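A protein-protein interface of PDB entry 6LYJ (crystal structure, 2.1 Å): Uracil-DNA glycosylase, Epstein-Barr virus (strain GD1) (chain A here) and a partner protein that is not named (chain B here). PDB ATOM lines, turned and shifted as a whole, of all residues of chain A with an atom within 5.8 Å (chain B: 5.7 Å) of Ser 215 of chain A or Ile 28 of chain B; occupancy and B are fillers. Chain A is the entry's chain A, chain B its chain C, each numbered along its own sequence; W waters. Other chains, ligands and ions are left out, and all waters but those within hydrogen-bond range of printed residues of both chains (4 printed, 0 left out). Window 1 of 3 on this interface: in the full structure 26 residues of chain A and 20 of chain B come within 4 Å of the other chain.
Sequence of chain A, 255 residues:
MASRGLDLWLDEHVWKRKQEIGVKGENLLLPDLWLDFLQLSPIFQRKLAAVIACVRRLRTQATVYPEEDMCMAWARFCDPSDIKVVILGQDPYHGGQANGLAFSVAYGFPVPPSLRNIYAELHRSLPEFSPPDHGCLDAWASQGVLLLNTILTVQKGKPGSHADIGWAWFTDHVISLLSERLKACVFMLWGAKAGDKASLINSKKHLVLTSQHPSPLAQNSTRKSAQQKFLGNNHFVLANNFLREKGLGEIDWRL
OE1 of Gln 90 of chain A lies within hydrogen-bond range of N of Glu 29 of chain B. The side-chain carboxylate of Glu 26 of chain B is in hydrogen-bond range of the side-chain hydroxyl of Ser 114 of chain A (2.4 Å). The backbone nitrogen of Pro 113 of chain A sits close to the side-chain carboxylate of Glu 26 of chain B (3.4 Å).
A ring nitrogen (ND1) of His 213 of chain A lies within hydrogen-bond range of the backbone NH of Ser 215 of chain A. The backbone NH (N) of Leu 217 of chain A lies close to the side-chain hydroxyl (OG) of Ser 215 of chain A, 3.2 Å away. The backbone NH (N) of Glu 26 of chain B is in hydrogen-bond range of the backbone carbonyl oxygen (O) of Thr 55 of chain B. The side-chain hydroxyl (OG) of Ser 27 of chain B is in hydrogen-bond range of the backbone carbonyl oxygen (O) of Thr 53 of chain B, at 3.1 Å. OG1 of Thr 53 of chain B is in hydrogen-bond range of O of Ile 28 of chain B (2.6 Å). The side-chain amide nitrogen (NE2) of Gln 52 of chain B sits at hydrogen-bond distance from the side-chain carboxylate (OE2) of Glu 29 of chain B (2.7 Å).
Among the printed residues, pairs that only touch across the chains: Gln 90 of chain A with Ile 28 of chain B (3.4 Å), His 213 of chain A with Ile 28 of chain B (3.4 Å), His 213 of chain A with Glu 30 of chain B (3.8 Å), Ser 215 of chain A with Ile 28 of chain B (3.7 Å), Leu 217 of chain A with Thr 53 of chain B (3.6 Å) and Leu 217 of chain A with Thr 55 of chain B (3.3 Å).
Printed residues of chain B within 4 Å of Pro 113 of chain A: Glu 26. Printed residues of chain B within 4 Å of Ser 114 of chain A: Glu 26 (2.4 Å). Printed residues of chain B within 4 Å of His 213 of chain A: Ile 28 and Glu 30. Ser 215 of chain A touches one residue of chain B. Of the printed residues of chain B, Leu 217 of chain A touches Thr 53 and Thr 55. Ser 27 of chain B touches none of the printed residues of chain A. Ile 28 of chain B touches three residues of chain A. Tyr 54 of chain B touches none of the printed residues of chain A.
Hydrophobic or aromatic side chains of chain B that line the printed part of chain A: Ile 28. Hydrophobic or aromatic side chains of chain A that line the printed part of chain B: Pro 113, His 213 and Leu 217. Among the printed residues, 9 pairs touch across the chains. Among the printed residues, no Asp or Glu carboxylate lies within 4 Å of a Lys or Arg side-chain nitrogen of the other chain.
Water W4 lies within hydrogen-bond range of the side-chain hydroxyl of Ser 215 of chain A (2.5 Å), the side-chain carboxylate of Glu 26 of chain B (2.7 Å) and the side-chain hydroxyl of Thr 55 of chain B (3.4 Å). Water W3 bridges OE1 of Gln 90 of chain A and OE1 of Glu 29 of chain B. Water W2 lies within hydrogen-bond range of the backbone carbonyl oxygen of Glu 29 of chain B, the side-chain carboxylate of Glu 30 of chain B and the side-chain amide nitrogen of Gln 90 of chain A. Water W1 lies within hydrogen-bond range of N of His 213 of chain A (2.8 Å) and OE2 of Glu 30 of chain B (2.9 Å).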
ATOM      1  N   GLN A  90     -11.380 -28.707 -28.392  1.00  0.00           N
ATOM      2  CA  GLN A  90     -11.843 -29.930 -29.039  1.00  0.00           C
ATOM      3  C   GLN A  90     -12.289 -29.621 -30.464  1.00  0.00           C
ATOM      4  O   GLN A  90     -11.464 -29.605 -31.382  1.00  0.00           O
ATOM      5  CB  GLN A  90     -12.976 -30.585 -28.234  1.00  0.00           C
ATOM      6  CG  GLN A  90     -12.527 -31.123 -26.876  1.00  0.00           C
ATOM      7  CD  GLN A  90     -13.667 -31.655 -26.020  1.00  0.00           C
ATOM      8  OE1 GLN A  90     -14.755 -31.953 -26.517  1.00  0.00           O
ATOM      9  NE2 GLN A  90     -13.418 -31.775 -24.720  1.00  0.00           N
ATOM     10  N   PRO A 113     -19.716 -20.337 -21.939  1.00  0.00           N
ATOM     11  CA  PRO A 113     -19.456 -20.604 -20.507  1.00  0.00           C
ATOM     12  C   PRO A 113     -18.006 -20.927 -20.174  1.00  0.00           C
ATOM     13  O   PRO A 113     -17.462 -20.393 -19.192  1.00  0.00           O
ATOM     14  CB  PRO A 113     -20.388 -21.790 -20.210  1.00  0.00           C
ATOM     15  CG  PRO A 113     -21.488 -21.668 -21.214  1.00  0.00           C
ATOM     16  CD  PRO A 113     -20.821 -21.159 -22.462  1.00  0.00           C
ATOM     17  N   SER A 114     -17.358 -21.789 -20.966  1.00  0.00           N
ATOM     18  CA  SER A 114     -15.967 -22.142 -20.686  1.00  0.00           C
ATOM     19  C   SER A 114     -15.065 -20.918 -20.771  1.00  0.00           C
ATOM     20  O   SER A 114     -14.117 -20.778 -19.989  1.00  0.00           O
ATOM     21  CB  SER A 114     -15.485 -23.225 -21.653  1.00  0.00           C
ATOM     22  OG  SER A 114     -16.110 -24.470 -21.396  1.00  0.00           O
ATOM     23  N   ASN A 117     -15.359 -18.935 -17.649  1.00  0.00           N
ATOM     24  CA  ASN A 117     -14.587 -19.495 -16.538  1.00  0.00           C
ATOM     25  C   ASN A 117     -13.084 -19.306 -16.731  1.00  0.00           C
ATOM     26  O   ASN A 117     -12.344 -19.135 -15.750  1.00  0.00           O
ATOM     27  CB  ASN A 117     -14.932 -20.969 -16.349  1.00  0.00           C
ATOM     28  CG  ASN A 117     -16.285 -21.162 -15.697  1.00  0.00           C
ATOM     29  OD1 ASN A 117     -16.827 -20.233 -15.099  1.00  0.00           O
ATOM     30  ND2 ASN A 117     -16.831 -22.373 -15.789  1.00  0.00           N
ATOM     31  N   HIS A 213     -11.317 -29.381 -17.010  1.00  0.00           N
ATOM     32  CA  HIS A 213     -11.815 -28.496 -18.046  1.00  0.00           C
ATOM     33  C   HIS A 213     -12.454 -27.259 -17.415  1.00  0.00           C
ATOM     34  O   HIS A 213     -13.016 -27.333 -16.321  1.00  0.00           O
ATOM     35  CB  HIS A 213     -12.835 -29.243 -18.901  1.00  0.00           C
ATOM     36  CG  HIS A 213     -13.091 -28.619 -20.236  1.00  0.00           C
ATOM     37  ND1 HIS A 213     -14.004 -27.604 -20.421  1.00  0.00           N
ATOM     38  CD2 HIS A 213     -12.557 -28.873 -21.454  1.00  0.00           C
ATOM     39  CE1 HIS A 213     -14.020 -27.258 -21.696  1.00  0.00           C
ATOM     40  NE2 HIS A 213     -13.154 -28.014 -22.345  1.00  0.00           N
ATOM     41  N   PRO A 214     -12.364 -26.099 -18.074  1.00  0.00           N
ATOM     42  CA  PRO A 214     -13.012 -24.894 -17.535  1.00  0.00           C
ATOM     43  C   PRO A 214     -14.529 -24.899 -17.630  1.00  0.00           C
ATOM     44  O   PRO A 214     -15.159 -23.964 -17.123  1.00  0.00           O
ATOM     45  CB  PRO A 214     -12.413 -23.773 -18.394  1.00  0.00           C
ATOM     46  CG  PRO A 214     -12.095 -24.451 -19.695  1.00  0.00           C
ATOM     47  CD  PRO A 214     -11.575 -25.798 -19.282  1.00  0.00           C
ATOM     48  N   SER A 215     -15.129 -25.903 -18.259  1.00  0.00           N
ATOM     49  CA  SER A 215     -16.577 -25.945 -18.406  1.00  0.00           C
ATOM     50  C   SER A 215     -17.258 -25.791 -17.045  1.00  0.00           C
ATOM     51  O   SER A 215     -16.791 -26.360 -16.049  1.00  0.00           O
ATOM     52  CB  SER A 215     -17.006 -27.262 -19.057  1.00  0.00           C
ATOM     53  OG  SER A 215     -18.416 -27.371 -19.107  1.00  0.00           O
ATOM     54  N   PRO A 216     -18.371 -25.057 -16.968  1.00  0.00           N
ATOM     55  CA  PRO A 216     -19.136 -25.021 -15.712  1.00  0.00           C
ATOM     56  C   PRO A 216     -19.623 -26.391 -15.274  1.00  0.00           C
ATOM     57  O   PRO A 216     -19.863 -26.592 -14.078  1.00  0.00           O
ATOM     58  CB  PRO A 216     -20.312 -24.093 -16.042  1.00  0.00           C
ATOM     59  CG  PRO A 216     -20.477 -24.219 -17.518  1.00  0.00           C
ATOM     60  CD  PRO A 216     -19.081 -24.378 -18.065  1.00  0.00           C
ATOM     61  N   LEU A 217     -19.772 -27.335 -16.207  1.00  0.00           N
ATOM     62  CA  LEU A 217     -20.159 -28.696 -15.846  1.00  0.00           C
ATOM     63  C   LEU A 217     -19.116 -29.365 -14.959  1.00  0.00           C
ATOM     64  O   LEU A 217     -19.465 -30.185 -14.101  1.00  0.00           O
ATOM     65  CB  LEU A 217     -20.383 -29.525 -17.111  1.00  0.00           C
ATOM     66  CG  LEU A 217     -21.461 -29.044 -18.084  1.00  0.00           C
ATOM     67  CD1 LEU A 217     -21.497 -29.932 -19.309  1.00  0.00           C
ATOM     68  CD2 LEU A 217     -22.825 -29.022 -17.412  1.00  0.00           C
ATOM     69  N   ALA A 218     -17.836 -29.055 -15.167  1.00  0.00           N
ATOM     70  CA  ALA A 218     -16.752 -29.631 -14.386  1.00  0.00           C
ATOM     71  C   ALA A 218     -16.317 -28.743 -13.227  1.00  0.00           C
ATOM     72  O   ALA A 218     -15.333 -29.063 -12.553  1.00  0.00           O
ATOM     73  CB  ALA A 218     -15.553 -29.923 -15.291  1.00  0.00           C
ATOM     74  N   GLN A 219     -17.018 -27.633 -12.984  1.00  0.00           N
ATOM     75  CA  GLN A 219     -16.530 -26.634 -12.036  1.00  0.00           C
ATOM     76  C   GLN A 219     -16.669 -27.123 -10.600  1.00  0.00           C
ATOM     77  O   GLN A 219     -15.674 -27.290  -9.886  1.00  0.00           O
ATOM     78  CB  GLN A 219     -17.272 -25.312 -12.228  1.00  0.00           C
ATOM     79  CG  GLN A 219     -16.942 -24.269 -11.171  1.00  0.00           C
ATOM     80  CD  GLN A 219     -17.067 -22.848 -11.685  1.00  0.00           C
ATOM     81  OE1 GLN A 219     -16.403 -22.461 -12.648  1.00  0.00           O
ATOM     82  NE2 GLN A 219     -17.923 -22.062 -11.042  1.00  0.00           N
ATOM     83  N   GLU B  26     -22.662 -24.594 -26.148  1.00  0.00           N
ATOM     84  CA  GLU B  26     -21.277 -25.044 -26.064  1.00  0.00           C
ATOM     85  C   GLU B  26     -21.261 -26.552 -25.840  1.00  0.00           C
ATOM     86  O   GLU B  26     -21.915 -27.050 -24.918  1.00  0.00           O
ATOM     87  CB  GLU B  26     -20.553 -24.328 -24.921  1.00  0.00           C
ATOM     88  CG  GLU B  26     -19.199 -24.902 -24.545  1.00  0.00           C
ATOM     89  CD  GLU B  26     -18.550 -24.139 -23.402  1.00  0.00           C
ATOM     90  OE1 GLU B  26     -18.253 -22.940 -23.576  1.00  0.00           O
ATOM     91  OE2 GLU B  26     -18.341 -24.735 -22.326  1.00  0.00           O
ATOM     92  N   SER B  27     -20.531 -27.276 -26.685  1.00  0.00           N
ATOM     93  CA  SER B  27     -20.418 -28.726 -26.582  1.00  0.00           C
ATOM     94  C   SER B  27     -18.973 -29.155 -26.371  1.00  0.00           C
ATOM     95  O   SER B  27     -18.090 -28.788 -27.155  1.00  0.00           O
ATOM     96  CB  SER B  27     -20.968 -29.412 -27.832  1.00  0.00           C
ATOM     97  OG  SER B  27     -22.373 -29.284 -27.914  1.00  0.00           O
ATOM     98  N   ILE B  28     -18.741 -29.950 -25.325  1.00  0.00           N
ATOM     99  CA  ILE B  28     -17.440 -30.551 -25.054  1.00  0.00           C
ATOM    100  C   ILE B  28     -17.673 -31.980 -24.581  1.00  0.00           C
ATOM    101  O   ILE B  28     -18.713 -32.300 -23.993  1.00  0.00           O
ATOM    102  CB  ILE B  28     -16.607 -29.774 -24.003  1.00  0.00           C
ATOM    103  CG1 ILE B  28     -17.249 -29.887 -22.623  1.00  0.00           C
ATOM    104  CG2 ILE B  28     -16.406 -28.305 -24.408  1.00  0.00           C
ATOM    105  CD1 ILE B  28     -16.258 -29.895 -21.500  1.00  0.00           C
ATOM    106  N   GLU B  29     -16.698 -32.846 -24.846  1.00  0.00           N
ATOM    107  CA  GLU B  29     -16.687 -34.198 -24.310  1.00  0.00           C
ATOM    108  C   GLU B  29     -15.851 -34.247 -23.041  1.00  0.00           C
ATOM    109  O   GLU B  29     -14.793 -33.615 -22.956  1.00  0.00           O
ATOM    110  CB  GLU B  29     -16.133 -35.193 -25.331  1.00  0.00           C
ATOM    111  CG  GLU B  29     -17.078 -35.502 -26.479  1.00  0.00           C
ATOM    112  CD  GLU B  29     -16.499 -36.532 -27.428  1.00  0.00           C
ATOM    113  OE1 GLU B  29     -15.354 -36.329 -27.877  1.00  0.00           O
ATOM    114  OE2 GLU B  29     -17.179 -37.538 -27.715  1.00  0.00           O
ATOM    115  N   GLU B  30     -16.333 -34.999 -22.055  1.00  0.00           N
ATOM    116  CA  GLU B  30     -15.602 -35.130 -20.800  1.00  0.00           C
ATOM    117  C   GLU B  30     -16.114 -36.361 -20.065  1.00  0.00           C
ATOM    118  O   GLU B  30     -17.270 -36.748 -20.227  1.00  0.00           O
ATOM    119  CB  GLU B  30     -15.752 -33.867 -19.940  1.00  0.00           C
ATOM    120  CG  GLU B  30     -14.952 -33.857 -18.648  1.00  0.00           C
ATOM    121  CD  GLU B  30     -13.460 -34.048 -18.873  1.00  0.00           C
ATOM    122  OE1 GLU B  30     -12.968 -35.177 -18.670  1.00  0.00           O
ATOM    123  OE2 GLU B  30     -12.778 -33.063 -19.230  1.00  0.00           O
ATOM    124  N   LEU B  51     -18.833 -38.531 -21.792  1.00  0.00           N
ATOM    125  CA  LEU B  51     -20.122 -37.970 -22.151  1.00  0.00           C
ATOM    126  C   LEU B  51     -19.931 -36.841 -23.155  1.00  0.00           C
ATOM    127  O   LEU B  51     -18.938 -36.101 -23.101  1.00  0.00           O
ATOM    128  CB  LEU B  51     -20.863 -37.454 -20.915  1.00  0.00           C
ATOM    129  CG  LEU B  51     -21.108 -38.460 -19.787  1.00  0.00           C
ATOM    130  CD1 LEU B  51     -21.973 -37.837 -18.698  1.00  0.00           C
ATOM    131  CD2 LEU B  51     -21.733 -39.747 -20.315  1.00  0.00           C
ATOM    132  N   GLN B  52     -20.872 -36.759 -24.096  1.00  0.00           N
ATOM    133  CA  GLN B  52     -21.031 -35.617 -24.986  1.00  0.00           C
ATOM    134  C   GLN B  52     -22.036 -34.665 -24.353  1.00  0.00           C
ATOM    135  O   GLN B  52     -23.127 -35.082 -23.949  1.00  0.00           O
ATOM    136  CB  GLN B  52     -21.507 -36.052 -26.375  1.00  0.00           C
ATOM    137  CG  GLN B  52     -20.532 -36.932 -27.162  1.00  0.00           C
ATOM    138  CD  GLN B  52     -20.440 -38.365 -26.640  1.00  0.00           C
ATOM    139  OE1 GLN B  52     -21.453 -38.984 -26.299  1.00  0.00           O
ATOM    140  NE2 GLN B  52     -19.223 -38.898 -26.587  1.00  0.00           N
ATOM    141  N   THR B  53     -21.667 -33.396 -24.246  1.00  0.00           N
ATOM    142  CA  THR B  53     -22.433 -32.449 -23.454  1.00  0.00           C
ATOM    143  C   THR B  53     -22.895 -31.270 -24.295  1.00  0.00           C
ATOM    144  O   THR B  53     -22.270 -30.914 -25.297  1.00  0.00           O
ATOM    145  CB  THR B  53     -21.608 -31.942 -22.276  1.00  0.00           C
ATOM    146  OG1 THR B  53     -20.585 -31.067 -22.761  1.00  0.00           O
ATOM    147  CG2 THR B  53     -20.955 -33.113 -21.546  1.00  0.00           C
ATOM    148  N   TYR B  54     -24.032 -30.703 -23.894  1.00  0.00           N
ATOM    149  CA  TYR B  54     -24.598 -29.493 -24.474  1.00  0.00           C
ATOM    150  C   TYR B  54     -24.923 -28.561 -23.319  1.00  0.00           C
ATOM    151  O   TYR B  54     -25.742 -28.910 -22.464  1.00  0.00           O
ATOM    152  CB  TYR B  54     -25.868 -29.786 -25.283  1.00  0.00           C
ATOM    153  CG  TYR B  54     -25.711 -30.780 -26.414  1.00  0.00           C
ATOM    154  CD1 TYR B  54     -25.568 -32.141 -26.157  1.00  0.00           C
ATOM    155  CD2 TYR B  54     -25.736 -30.361 -27.739  1.00  0.00           C
ATOM    156  CE1 TYR B  54     -25.433 -33.051 -27.189  1.00  0.00           C
ATOM    157  CE2 TYR B  54     -25.604 -31.264 -28.774  1.00  0.00           C
ATOM    158  CZ  TYR B  54     -25.452 -32.607 -28.495  1.00  0.00           C
ATOM    159  OH  TYR B  54     -25.318 -33.507 -29.526  1.00  0.00           O
ATOM    160  N   THR B  55     -24.278 -27.399 -23.275  1.00  0.00           N
ATOM    161  CA  THR B  55     -24.559 -26.391 -22.260  1.00  0.00           C
ATOM    162  C   THR B  55     -25.038 -25.131 -22.958  1.00  0.00           C
ATOM    163  O   THR B  55     -24.350 -24.605 -23.838  1.00  0.00           O
ATOM    164  CB  THR B  55     -23.320 -26.091 -21.409  1.00  0.00           C
ATOM    165  OG1 THR B  55     -22.844 -27.300 -20.804  1.00  0.00           O
ATOM    166  CG2 THR B  55     -23.640 -25.061 -20.326  1.00  0.00           C
HETATM  167  O   HOH W   1     -12.462 -31.862 -16.621  1.00  0.00           O
HETATM  168  O   HOH W   2     -12.336 -33.418 -21.991  1.00  0.00           O
HETATM  169  O   HOH W   3     -14.451 -33.867 -28.308  1.00  0.00           O
HETATM  170  O   HOH W   4     -19.537 -26.896 -21.275  1.00  0.00           O
